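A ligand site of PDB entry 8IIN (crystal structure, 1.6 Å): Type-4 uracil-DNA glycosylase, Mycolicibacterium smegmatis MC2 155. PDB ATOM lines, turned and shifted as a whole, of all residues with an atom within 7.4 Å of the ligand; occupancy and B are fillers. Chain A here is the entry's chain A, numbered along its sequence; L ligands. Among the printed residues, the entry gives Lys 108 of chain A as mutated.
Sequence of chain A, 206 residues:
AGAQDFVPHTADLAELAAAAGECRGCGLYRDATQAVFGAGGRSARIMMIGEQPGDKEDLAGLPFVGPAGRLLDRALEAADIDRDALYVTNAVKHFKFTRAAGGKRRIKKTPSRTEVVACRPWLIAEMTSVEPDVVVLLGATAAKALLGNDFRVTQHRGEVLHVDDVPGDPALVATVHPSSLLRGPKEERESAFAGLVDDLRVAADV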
ATOM      1  N   VAL A  36      12.292  28.391 -35.621  1.00  0.00           N
ATOM      2  CA  VAL A  36      13.642  27.942 -35.182  1.00  0.00           C
ATOM      3  C   VAL A  36      13.424  26.588 -34.534  1.00  0.00           C
ATOM      4  O   VAL A  36      12.882  26.504 -33.434  1.00  0.00           O
ATOM      5  CB  VAL A  36      14.291  28.949 -34.226  1.00  0.00           C
ATOM      6  CG1 VAL A  36      15.624  28.446 -33.703  1.00  0.00           C
ATOM      7  CG2 VAL A  36      14.461  30.306 -34.890  1.00  0.00           C
ATOM      8  N   ILE A  49      15.645  22.230 -23.305  1.00  0.00           N
ATOM      9  CA  ILE A  49      14.515  23.023 -23.843  1.00  0.00           C
ATOM     10  C   ILE A  49      14.497  24.403 -23.185  1.00  0.00           C
ATOM     11  O   ILE A  49      14.419  24.482 -21.988  1.00  0.00           O
ATOM     12  CB  ILE A  49      13.187  22.296 -23.611  1.00  0.00           C
ATOM     13  CG1 ILE A  49      13.220  20.841 -24.073  1.00  0.00           C
ATOM     14  CG2 ILE A  49      12.038  23.054 -24.245  1.00  0.00           C
ATOM     15  CD1 ILE A  49      11.923  20.113 -23.895  1.00  0.00           C
ATOM     16  N   GLY A  50      14.579  25.429 -24.010  1.00  0.00           N
ATOM     17  CA  GLY A  50      14.454  26.813 -23.517  1.00  0.00           C
ATOM     18  C   GLY A  50      13.064  27.345 -23.800  1.00  0.00           C
ATOM     19  O   GLY A  50      12.185  26.560 -24.077  1.00  0.00           O
ATOM     20  N   GLU A  51      12.906  28.661 -23.749  1.00  0.00           N
ATOM     21  CA  GLU A  51      11.536  29.221 -23.865  1.00  0.00           C
ATOM     22  C   GLU A  51      11.175  29.422 -25.339  1.00  0.00           C
ATOM     23  O   GLU A  51      10.184  28.867 -25.766  1.00  0.00           O
ATOM     24  CB  GLU A  51      11.562  30.593 -23.183  1.00  0.00           C
ATOM     25  CG  GLU A  51      10.269  31.362 -23.329  1.00  0.00           C
ATOM     26  CD  GLU A  51      10.212  32.625 -22.487  1.00  0.00           C
ATOM     27  OE1 GLU A  51      10.673  33.673 -22.975  1.00  0.00           O
ATOM     28  OE2 GLU A  51       9.713  32.549 -21.364  1.00  0.00           O
ATOM     29  N   GLN A  52      12.008  30.184 -26.026  1.00  0.00           N
ATOM     30  CA  GLN A  52      11.737  30.566 -27.430  1.00  0.00           C
ATOM     31  C   GLN A  52      13.013  31.118 -28.044  1.00  0.00           C
ATOM     32  O   GLN A  52      13.903  31.519 -27.316  1.00  0.00           O
ATOM     33  CB  GLN A  52      10.670  31.668 -27.488  1.00  0.00           C
ATOM     34  CG  GLN A  52      11.095  32.930 -26.771  1.00  0.00           C
ATOM     35  CD  GLN A  52      10.094  34.047 -26.896  1.00  0.00           C
ATOM     36  OE1 GLN A  52       9.702  34.408 -27.991  1.00  0.00           O
ATOM     37  NE2 GLN A  52       9.684  34.595 -25.766  1.00  0.00           N
ATOM     38  N   PRO A  53      13.125  31.126 -29.372  1.00  0.00           N
ATOM     39  CA  PRO A  53      14.251  31.794 -29.975  1.00  0.00           C
ATOM     40  C   PRO A  53      14.146  33.284 -29.656  1.00  0.00           C
ATOM     41  O   PRO A  53      13.061  33.761 -29.594  1.00  0.00           O
ATOM     42  CB  PRO A  53      13.998  31.598 -31.480  1.00  0.00           C
ATOM     43  CG  PRO A  53      12.531  31.286 -31.600  1.00  0.00           C
ATOM     44  CD  PRO A  53      12.223  30.502 -30.349  1.00  0.00           C
ATOM     45  N   GLY A  54      15.285  33.925 -29.445  1.00  0.00           N
ATOM     46  CA  GLY A  54      15.298  35.376 -29.274  1.00  0.00           C
ATOM     47  C   GLY A  54      15.665  36.091 -30.564  1.00  0.00           C
ATOM     48  O   GLY A  54      15.586  35.501 -31.602  1.00  0.00           O
ATOM     49  N   ASP A  55      16.083  37.342 -30.430  1.00  0.00           N
ATOM     50  CA  ASP A  55      16.414  38.188 -31.617  1.00  0.00           C
ATOM     51  C   ASP A  55      17.486  37.519 -32.493  1.00  0.00           C
ATOM     52  O   ASP A  55      17.279  37.411 -33.703  1.00  0.00           O
ATOM     53  CB  ASP A  55      16.841  39.570 -31.122  1.00  0.00           C
ATOM     54  CG  ASP A  55      17.044  40.645 -32.186  1.00  0.00           C
ATOM     55  OD1 ASP A  55      16.872  40.350 -33.359  1.00  0.00           O
ATOM     56  OD2 ASP A  55      17.369  41.761 -31.811  1.00  0.00           O
ATOM     57  N   GLU A  57      18.548  34.391 -32.542  1.00  0.00           N
ATOM     58  CA  GLU A  57      18.149  33.050 -33.036  1.00  0.00           C
ATOM     59  C   GLU A  57      17.130  33.159 -34.173  1.00  0.00           C
ATOM     60  O   GLU A  57      17.166  32.344 -35.068  1.00  0.00           O
ATOM     61  CB  GLU A  57      17.473  32.269 -31.896  1.00  0.00           C
ATOM     62  CG  GLU A  57      18.405  31.849 -30.779  1.00  0.00           C
ATOM     63  CD  GLU A  57      18.849  32.924 -29.802  1.00  0.00           C
ATOM     64  OE1 GLU A  57      18.170  33.939 -29.710  1.00  0.00           O
ATOM     65  OE2 GLU A  57      19.865  32.724 -29.137  1.00  0.00           O
ATOM     66  N   LEU A  62      18.874  29.083 -35.552  1.00  0.00           N
ATOM     67  CA  LEU A  62      19.480  28.123 -34.639  1.00  0.00           C
ATOM     68  C   LEU A  62      19.184  28.571 -33.217  1.00  0.00           C
ATOM     69  O   LEU A  62      19.124  29.771 -32.943  1.00  0.00           O
ATOM     70  CB  LEU A  62      21.011  28.079 -34.819  1.00  0.00           C
ATOM     71  CG  LEU A  62      21.493  27.500 -36.134  1.00  0.00           C
ATOM     72  CD1 LEU A  62      22.977  27.785 -36.308  1.00  0.00           C
ATOM     73  CD2 LEU A  62      21.207  26.018 -36.162  1.00  0.00           C
ATOM     74  N   PRO A  63      19.026  27.636 -32.282  1.00  0.00           N
ATOM     75  CA  PRO A  63      18.789  28.031 -30.899  1.00  0.00           C
ATOM     76  C   PRO A  63      20.077  28.418 -30.184  1.00  0.00           C
ATOM     77  O   PRO A  63      21.179  27.986 -30.565  1.00  0.00           O
ATOM     78  CB  PRO A  63      18.181  26.778 -30.252  1.00  0.00           C
ATOM     79  CG  PRO A  63      18.678  25.637 -31.099  1.00  0.00           C
ATOM     80  CD  PRO A  63      18.981  26.175 -32.484  1.00  0.00           C
ATOM     81  N   PHE A  64      19.906  29.230 -29.150  1.00  0.00           N
ATOM     82  CA  PHE A  64      20.937  29.593 -28.166  1.00  0.00           C
ATOM     83  C   PHE A  64      22.243  30.032 -28.834  1.00  0.00           C
ATOM     84  O   PHE A  64      23.305  29.435 -28.656  1.00  0.00           O
ATOM     85  CB  PHE A  64      21.144  28.438 -27.169  1.00  0.00           C
ATOM     86  CG  PHE A  64      20.097  28.391 -26.080  1.00  0.00           C
ATOM     87  CD1 PHE A  64      20.043  29.389 -25.115  1.00  0.00           C
ATOM     88  CD2 PHE A  64      19.146  27.389 -26.063  1.00  0.00           C
ATOM     89  CE1 PHE A  64      19.049  29.362 -24.119  1.00  0.00           C
ATOM     90  CE2 PHE A  64      18.159  27.356 -25.082  1.00  0.00           C
ATOM     91  CZ  PHE A  64      18.111  28.343 -24.110  1.00  0.00           C
ATOM     92  N   VAL A  65      22.142  31.118 -29.596  1.00  0.00           N
ATOM     93  CA  VAL A  65      23.303  31.703 -30.270  1.00  0.00           C
ATOM     94  C   VAL A  65      23.664  33.073 -29.744  1.00  0.00           C
ATOM     95  O   VAL A  65      24.714  33.617 -30.130  1.00  0.00           O
ATOM     96  CB  VAL A  65      23.107  31.762 -31.806  1.00  0.00           C
ATOM     97  CG1 VAL A  65      23.028  30.353 -32.392  1.00  0.00           C
ATOM     98  CG2 VAL A  65      21.891  32.603 -32.165  1.00  0.00           C
ATOM     99  N   GLY A  66      22.848  33.659 -28.880  1.00  0.00           N
ATOM    100  CA  GLY A  66      23.110  34.967 -28.346  1.00  0.00           C
ATOM    101  C   GLY A  66      23.800  34.899 -26.999  1.00  0.00           C
ATOM    102  O   GLY A  66      24.415  33.896 -26.648  1.00  0.00           O
ATOM    103  N   PRO A  67      23.710  35.993 -26.236  1.00  0.00           N
ATOM    104  CA  PRO A  67      24.395  36.049 -24.932  1.00  0.00           C
ATOM    105  C   PRO A  67      24.009  34.932 -23.993  1.00  0.00           C
ATOM    106  O   PRO A  67      24.869  34.399 -23.274  1.00  0.00           O
ATOM    107  CB  PRO A  67      23.961  37.413 -24.379  1.00  0.00           C
ATOM    108  CG  PRO A  67      23.767  38.237 -25.614  1.00  0.00           C
ATOM    109  CD  PRO A  67      23.087  37.292 -26.576  1.00  0.00           C
ATOM    110  N   ALA A  68      22.720  34.578 -23.947  1.00  0.00           N
ATOM    111  CA  ALA A  68      22.295  33.484 -23.082  1.00  0.00           C
ATOM    112  C   ALA A  68      22.917  32.173 -23.541  1.00  0.00           C
ATOM    113  O   ALA A  68      23.311  31.339 -22.709  1.00  0.00           O
ATOM    114  CB  ALA A  68      20.765  33.385 -23.065  1.00  0.00           C
ATOM    115  N   GLY A  69      23.019  31.966 -24.868  1.00  0.00           N
ATOM    116  CA  GLY A  69      23.669  30.780 -25.395  1.00  0.00           C
ATOM    117  C   GLY A  69      25.154  30.712 -25.061  1.00  0.00           C
ATOM    118  O   GLY A  69      25.699  29.635 -24.825  1.00  0.00           O
ATOM    119  N   ARG A  83      28.232  20.174 -26.177  1.00  0.00           N
ATOM    120  CA  ARG A  83      26.988  20.763 -26.760  1.00  0.00           C
ATOM    121  C   ARG A  83      26.663  20.055 -28.074  1.00  0.00           C
ATOM    122  O   ARG A  83      25.477  19.942 -28.434  1.00  0.00           O
ATOM    123  CB  ARG A  83      27.112  22.270 -27.006  1.00  0.00           C
ATOM    124  CG  ARG A  83      25.797  22.900 -27.446  1.00  0.00           C
ATOM    125  CD  ARG A  83      25.814  24.396 -27.600  1.00  0.00           C
ATOM    126  NE  ARG A  83      24.680  24.869 -28.375  1.00  0.00           N
ATOM    127  CZ  ARG A  83      24.250  26.125 -28.379  1.00  0.00           C
ATOM    128  NH1 ARG A  83      24.853  27.036 -27.647  1.00  0.00           N
ATOM    129  NH2 ARG A  83      23.215  26.453 -29.128  1.00  0.00           N
ATOM    130  N   VAL A  88      19.053  20.487 -28.643  1.00  0.00           N
ATOM    131  CA  VAL A  88      18.709  21.739 -27.994  1.00  0.00           C
ATOM    132  C   VAL A  88      17.556  22.379 -28.748  1.00  0.00           C
ATOM    133  O   VAL A  88      17.636  22.560 -29.969  1.00  0.00           O
ATOM    134  CB  VAL A  88      19.922  22.692 -27.933  1.00  0.00           C
ATOM    135  CG1 VAL A  88      19.517  24.045 -27.376  1.00  0.00           C
ATOM    136  CG2 VAL A  88      21.053  22.065 -27.113  1.00  0.00           C
ATOM    137  N   THR A  89      16.495  22.739 -28.032  1.00  0.00           N
ATOM    138  CA  THR A  89      15.303  23.291 -28.698  1.00  0.00           C
ATOM    139  C   THR A  89      14.623  24.248 -27.717  1.00  0.00           C
ATOM    140  O   THR A  89      15.211  24.648 -26.709  1.00  0.00           O
ATOM    141  CB  THR A  89      14.391  22.156 -29.191  1.00  0.00           C
ATOM    142  OG1 THR A  89      13.387  22.709 -30.066  1.00  0.00           O
ATOM    143  CG2 THR A  89      13.729  21.394 -28.033  1.00  0.00           C
ATOM    144  N   ASN A  90      13.394  24.650 -28.054  1.00  0.00           N
ATOM    145  CA  ASN A  90      12.626  25.644 -27.272  1.00  0.00           C
ATOM    146  C   ASN A  90      11.166  25.210 -27.207  1.00  0.00           C
ATOM    147  O   ASN A  90      10.707  24.520 -28.113  1.00  0.00           O
ATOM    148  CB  ASN A  90      12.710  27.015 -27.933  1.00  0.00           C
ATOM    149  CG  ASN A  90      14.069  27.628 -27.747  1.00  0.00           C
ATOM    150  OD1 ASN A  90      14.453  27.905 -26.620  1.00  0.00           O
ATOM    151  ND2 ASN A  90      14.826  27.780 -28.822  1.00  0.00           N
ATOM    152  N   ALA A  91      10.468  25.660 -26.163  1.00  0.00           N
ATOM    153  CA  ALA A  91       9.041  25.297 -25.985  1.00  0.00           C
ATOM    154  C   ALA A  91       8.212  25.911 -27.120  1.00  0.00           C
ATOM    155  O   ALA A  91       7.253  25.281 -27.562  1.00  0.00           O
ATOM    156  CB  ALA A  91       8.577  25.774 -24.644  1.00  0.00           C
ATOM    157  N   VAL A  92       8.562  27.141 -27.498  1.00  0.00           N
ATOM    158  CA  VAL A  92       7.875  27.873 -28.587  1.00  0.00           C
ATOM    159  C   VAL A  92       8.917  28.079 -29.708  1.00  0.00           C
ATOM    160  O   VAL A  92      10.060  28.346 -29.359  1.00  0.00           O
ATOM    161  CB  VAL A  92       7.243  29.155 -28.026  1.00  0.00           C
ATOM    162  CG1 VAL A  92       6.859  30.160 -29.091  1.00  0.00           C
ATOM    163  CG2 VAL A  92       6.032  28.799 -27.175  1.00  0.00           C
ATOM    164  N   LYS A 108      12.082  40.172 -26.294  1.00  0.00           N
ATOM    165  CA  LYS A 108      11.192  38.976 -26.172  1.00  0.00           C
ATOM    166  C   LYS A 108       9.919  39.336 -25.409  1.00  0.00           C
ATOM    167  O   LYS A 108      10.071  40.020 -24.393  1.00  0.00           O
ATOM    168  CB  LYS A 108      11.832  37.875 -25.318  1.00  0.00           C
ATOM    169  CG  LYS A 108      12.559  36.756 -26.037  1.00  0.00           C
ATOM    170  CD  LYS A 108      13.400  35.982 -25.072  1.00  0.00           C
ATOM    171  CE  LYS A 108      14.610  35.327 -25.694  1.00  0.00           C
ATOM    172  NZ  LYS A 108      14.332  33.914 -26.028  1.00  0.00           N
ATOM    173  N   LEU A 138      15.050  24.638 -19.221  1.00  0.00           N
ATOM    174  CA  LEU A 138      15.733  25.900 -18.878  1.00  0.00           C
ATOM    175  C   LEU A 138      14.705  26.994 -18.698  1.00  0.00           C
ATOM    176  O   LEU A 138      14.244  27.530 -19.710  1.00  0.00           O
ATOM    177  CB  LEU A 138      16.677  26.251 -20.024  1.00  0.00           C
ATOM    178  CG  LEU A 138      17.765  25.228 -20.337  1.00  0.00           C
ATOM    179  CD1 LEU A 138      18.406  25.509 -21.683  1.00  0.00           C
ATOM    180  CD2 LEU A 138      18.831  25.233 -19.256  1.00  0.00           C
ATOM    181  N   ALA A 142       9.525  26.627 -20.268  1.00  0.00           N
ATOM    182  CA  ALA A 142       9.874  25.241 -20.652  1.00  0.00           C
ATOM    183  C   ALA A 142       9.440  24.234 -19.578  1.00  0.00           C
ATOM    184  O   ALA A 142       8.926  23.188 -19.898  1.00  0.00           O
ATOM    185  CB  ALA A 142      11.375  25.136 -20.860  1.00  0.00           C
ATOM    186  N   HIS A 177      16.915  29.651 -16.277  1.00  0.00           N
ATOM    187  CA  HIS A 177      17.227  30.004 -17.673  1.00  0.00           C
ATOM    188  C   HIS A 177      18.547  30.765 -17.692  1.00  0.00           C
ATOM    189  O   HIS A 177      18.740  31.626 -16.856  1.00  0.00           O
ATOM    190  CB  HIS A 177      16.121  30.903 -18.192  1.00  0.00           C
ATOM    191  CG  HIS A 177      16.166  31.027 -19.669  1.00  0.00           C
ATOM    192  ND1 HIS A 177      17.078  31.848 -20.298  1.00  0.00           N
ATOM    193  CD2 HIS A 177      15.491  30.401 -20.638  1.00  0.00           C
ATOM    194  CE1 HIS A 177      16.946  31.738 -21.595  1.00  0.00           C
ATOM    195  NE2 HIS A 177      15.985  30.860 -21.828  1.00  0.00           N
ATOM    196  N   PRO A 178      19.483  30.441 -18.608  1.00  0.00           N
ATOM    197  CA  PRO A 178      20.760  31.124 -18.660  1.00  0.00           C
ATOM    198  C   PRO A 178      20.663  32.656 -18.730  1.00  0.00           C
ATOM    199  O   PRO A 178      21.561  33.284 -18.274  1.00  0.00           O
ATOM    200  CB  PRO A 178      21.464  30.485 -19.870  1.00  0.00           C
ATOM    201  CG  PRO A 178      20.362  29.846 -20.664  1.00  0.00           C
ATOM    202  CD  PRO A 178      19.386  29.384 -19.608  1.00  0.00           C
ATOM    203  N   SER A 179      19.572  33.183 -19.285  1.00  0.00           N
ATOM    204  CA  SER A 179      19.407  34.657 -19.407  1.00  0.00           C
ATOM    205  C   SER A 179      19.315  35.290 -18.022  1.00  0.00           C
ATOM    206  O   SER A 179      19.664  36.452 -17.875  1.00  0.00           O
ATOM    207  CB  SER A 179      18.220  35.055 -20.242  1.00  0.00           C
ATOM    208  OG  SER A 179      17.013  34.746 -19.573  1.00  0.00           O
HETATM  209  N1  LIG L   1      16.574  31.964 -25.019  1.00  0.00           N
HETATM  210  C1  LIG L   1      15.860  30.811 -25.158  1.00  0.00           C
HETATM  211  O1  LIG L   1      14.995  30.460 -24.364  1.00  0.00           O
HETATM  212  N2  LIG L   1      16.153  30.064 -26.253  1.00  0.00           N
HETATM  213  C2  LIG L   1      17.069  30.372 -27.236  1.00  0.00           C
HETATM  214  O2  LIG L   1      17.227  29.600 -28.170  1.00  0.00           O
HETATM  215  C3  LIG L   1      17.774  31.588 -26.993  1.00  0.00           C
HETATM  216  C4  LIG L   1      17.517  32.336 -25.909  1.00  0.00           C
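The backbone carbonyl oxygen (O) of Gln 52 sits at hydrogen-bond distance from a nitrogen (N2) of the ligand, at 2.9 Å.
An oxygen (O2) of the ligand lies within hydrogen-bond range of the backbone NH (N) of Phe 64 (2.9 Å).
An oxygen (O1) of the ligand lies within hydrogen-bond range of the backbone NH (N) of Gln 52, at 3.4 Å.
The backbone NH of Glu 51 lies within hydrogen-bond range of an oxygen (O1) of the ligand (2.8 Å).
OD1 of Asn 90 sits at hydrogen-bond distance from N2 of the ligand.
NE2 of His 177 sits at hydrogen-bond distance from O1 of the ligand (2.8 Å).
The side-chain amino group (NZ) of Lys 108 sits close to a nitrogen (N1) of the ligand.
Residues that only touch the ligand: Glu 57 (3.2 Å), Pro 63 (3.5 Å) and Gly 50 (3.7 Å).
Hydrophobic or aromatic side chains within 4 Å of the ligand: Pro 63, Phe 64 and His 177.
Within 4 Å of the ligand: Gly 50, Glu 51, Gln 52, Glu 57, Pro 63, Phe 64, Asn 90, Lys 108 and His 177.
Along chain A the residues within 4 Å of the ligand span positions 50 to 177.
The nearest printed residue that does not touch the ligand is Pro 53 (4.1 Å).
N of Phe 64 sits close to OE2 of Glu 57 (3.5 Å).
The side-chain carboxylate (OE2) of Glu 57 is in hydrogen-bond range of the backbone NH (N) of Val 65 (2.8 Å).
NZ of Lys 108 is in hydrogen-bond range of O of Gln 52, at 2.8 Å.
The backbone carbonyl oxygen (O) of Gly 50 sits at hydrogen-bond distance from the backbone NH (N) of Ala 91 (2.8 Å).
N of Gly 54 is in hydrogen-bond range of OE1 of Glu 57, 2.9 Å away.
N of Ala 91 sits at hydrogen-bond distance from O of Glu 51 (3.2 Å).
The side-chain amide oxygen (OD1) of Asn 90 lies within hydrogen-bond range of the backbone NH (N) of Gln 52.
The side-chain carboxylate (OE1) of Glu 51 sits at hydrogen-bond distance from the side-chain amide nitrogen (NE2) of Gln 52 (3.1 Å).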
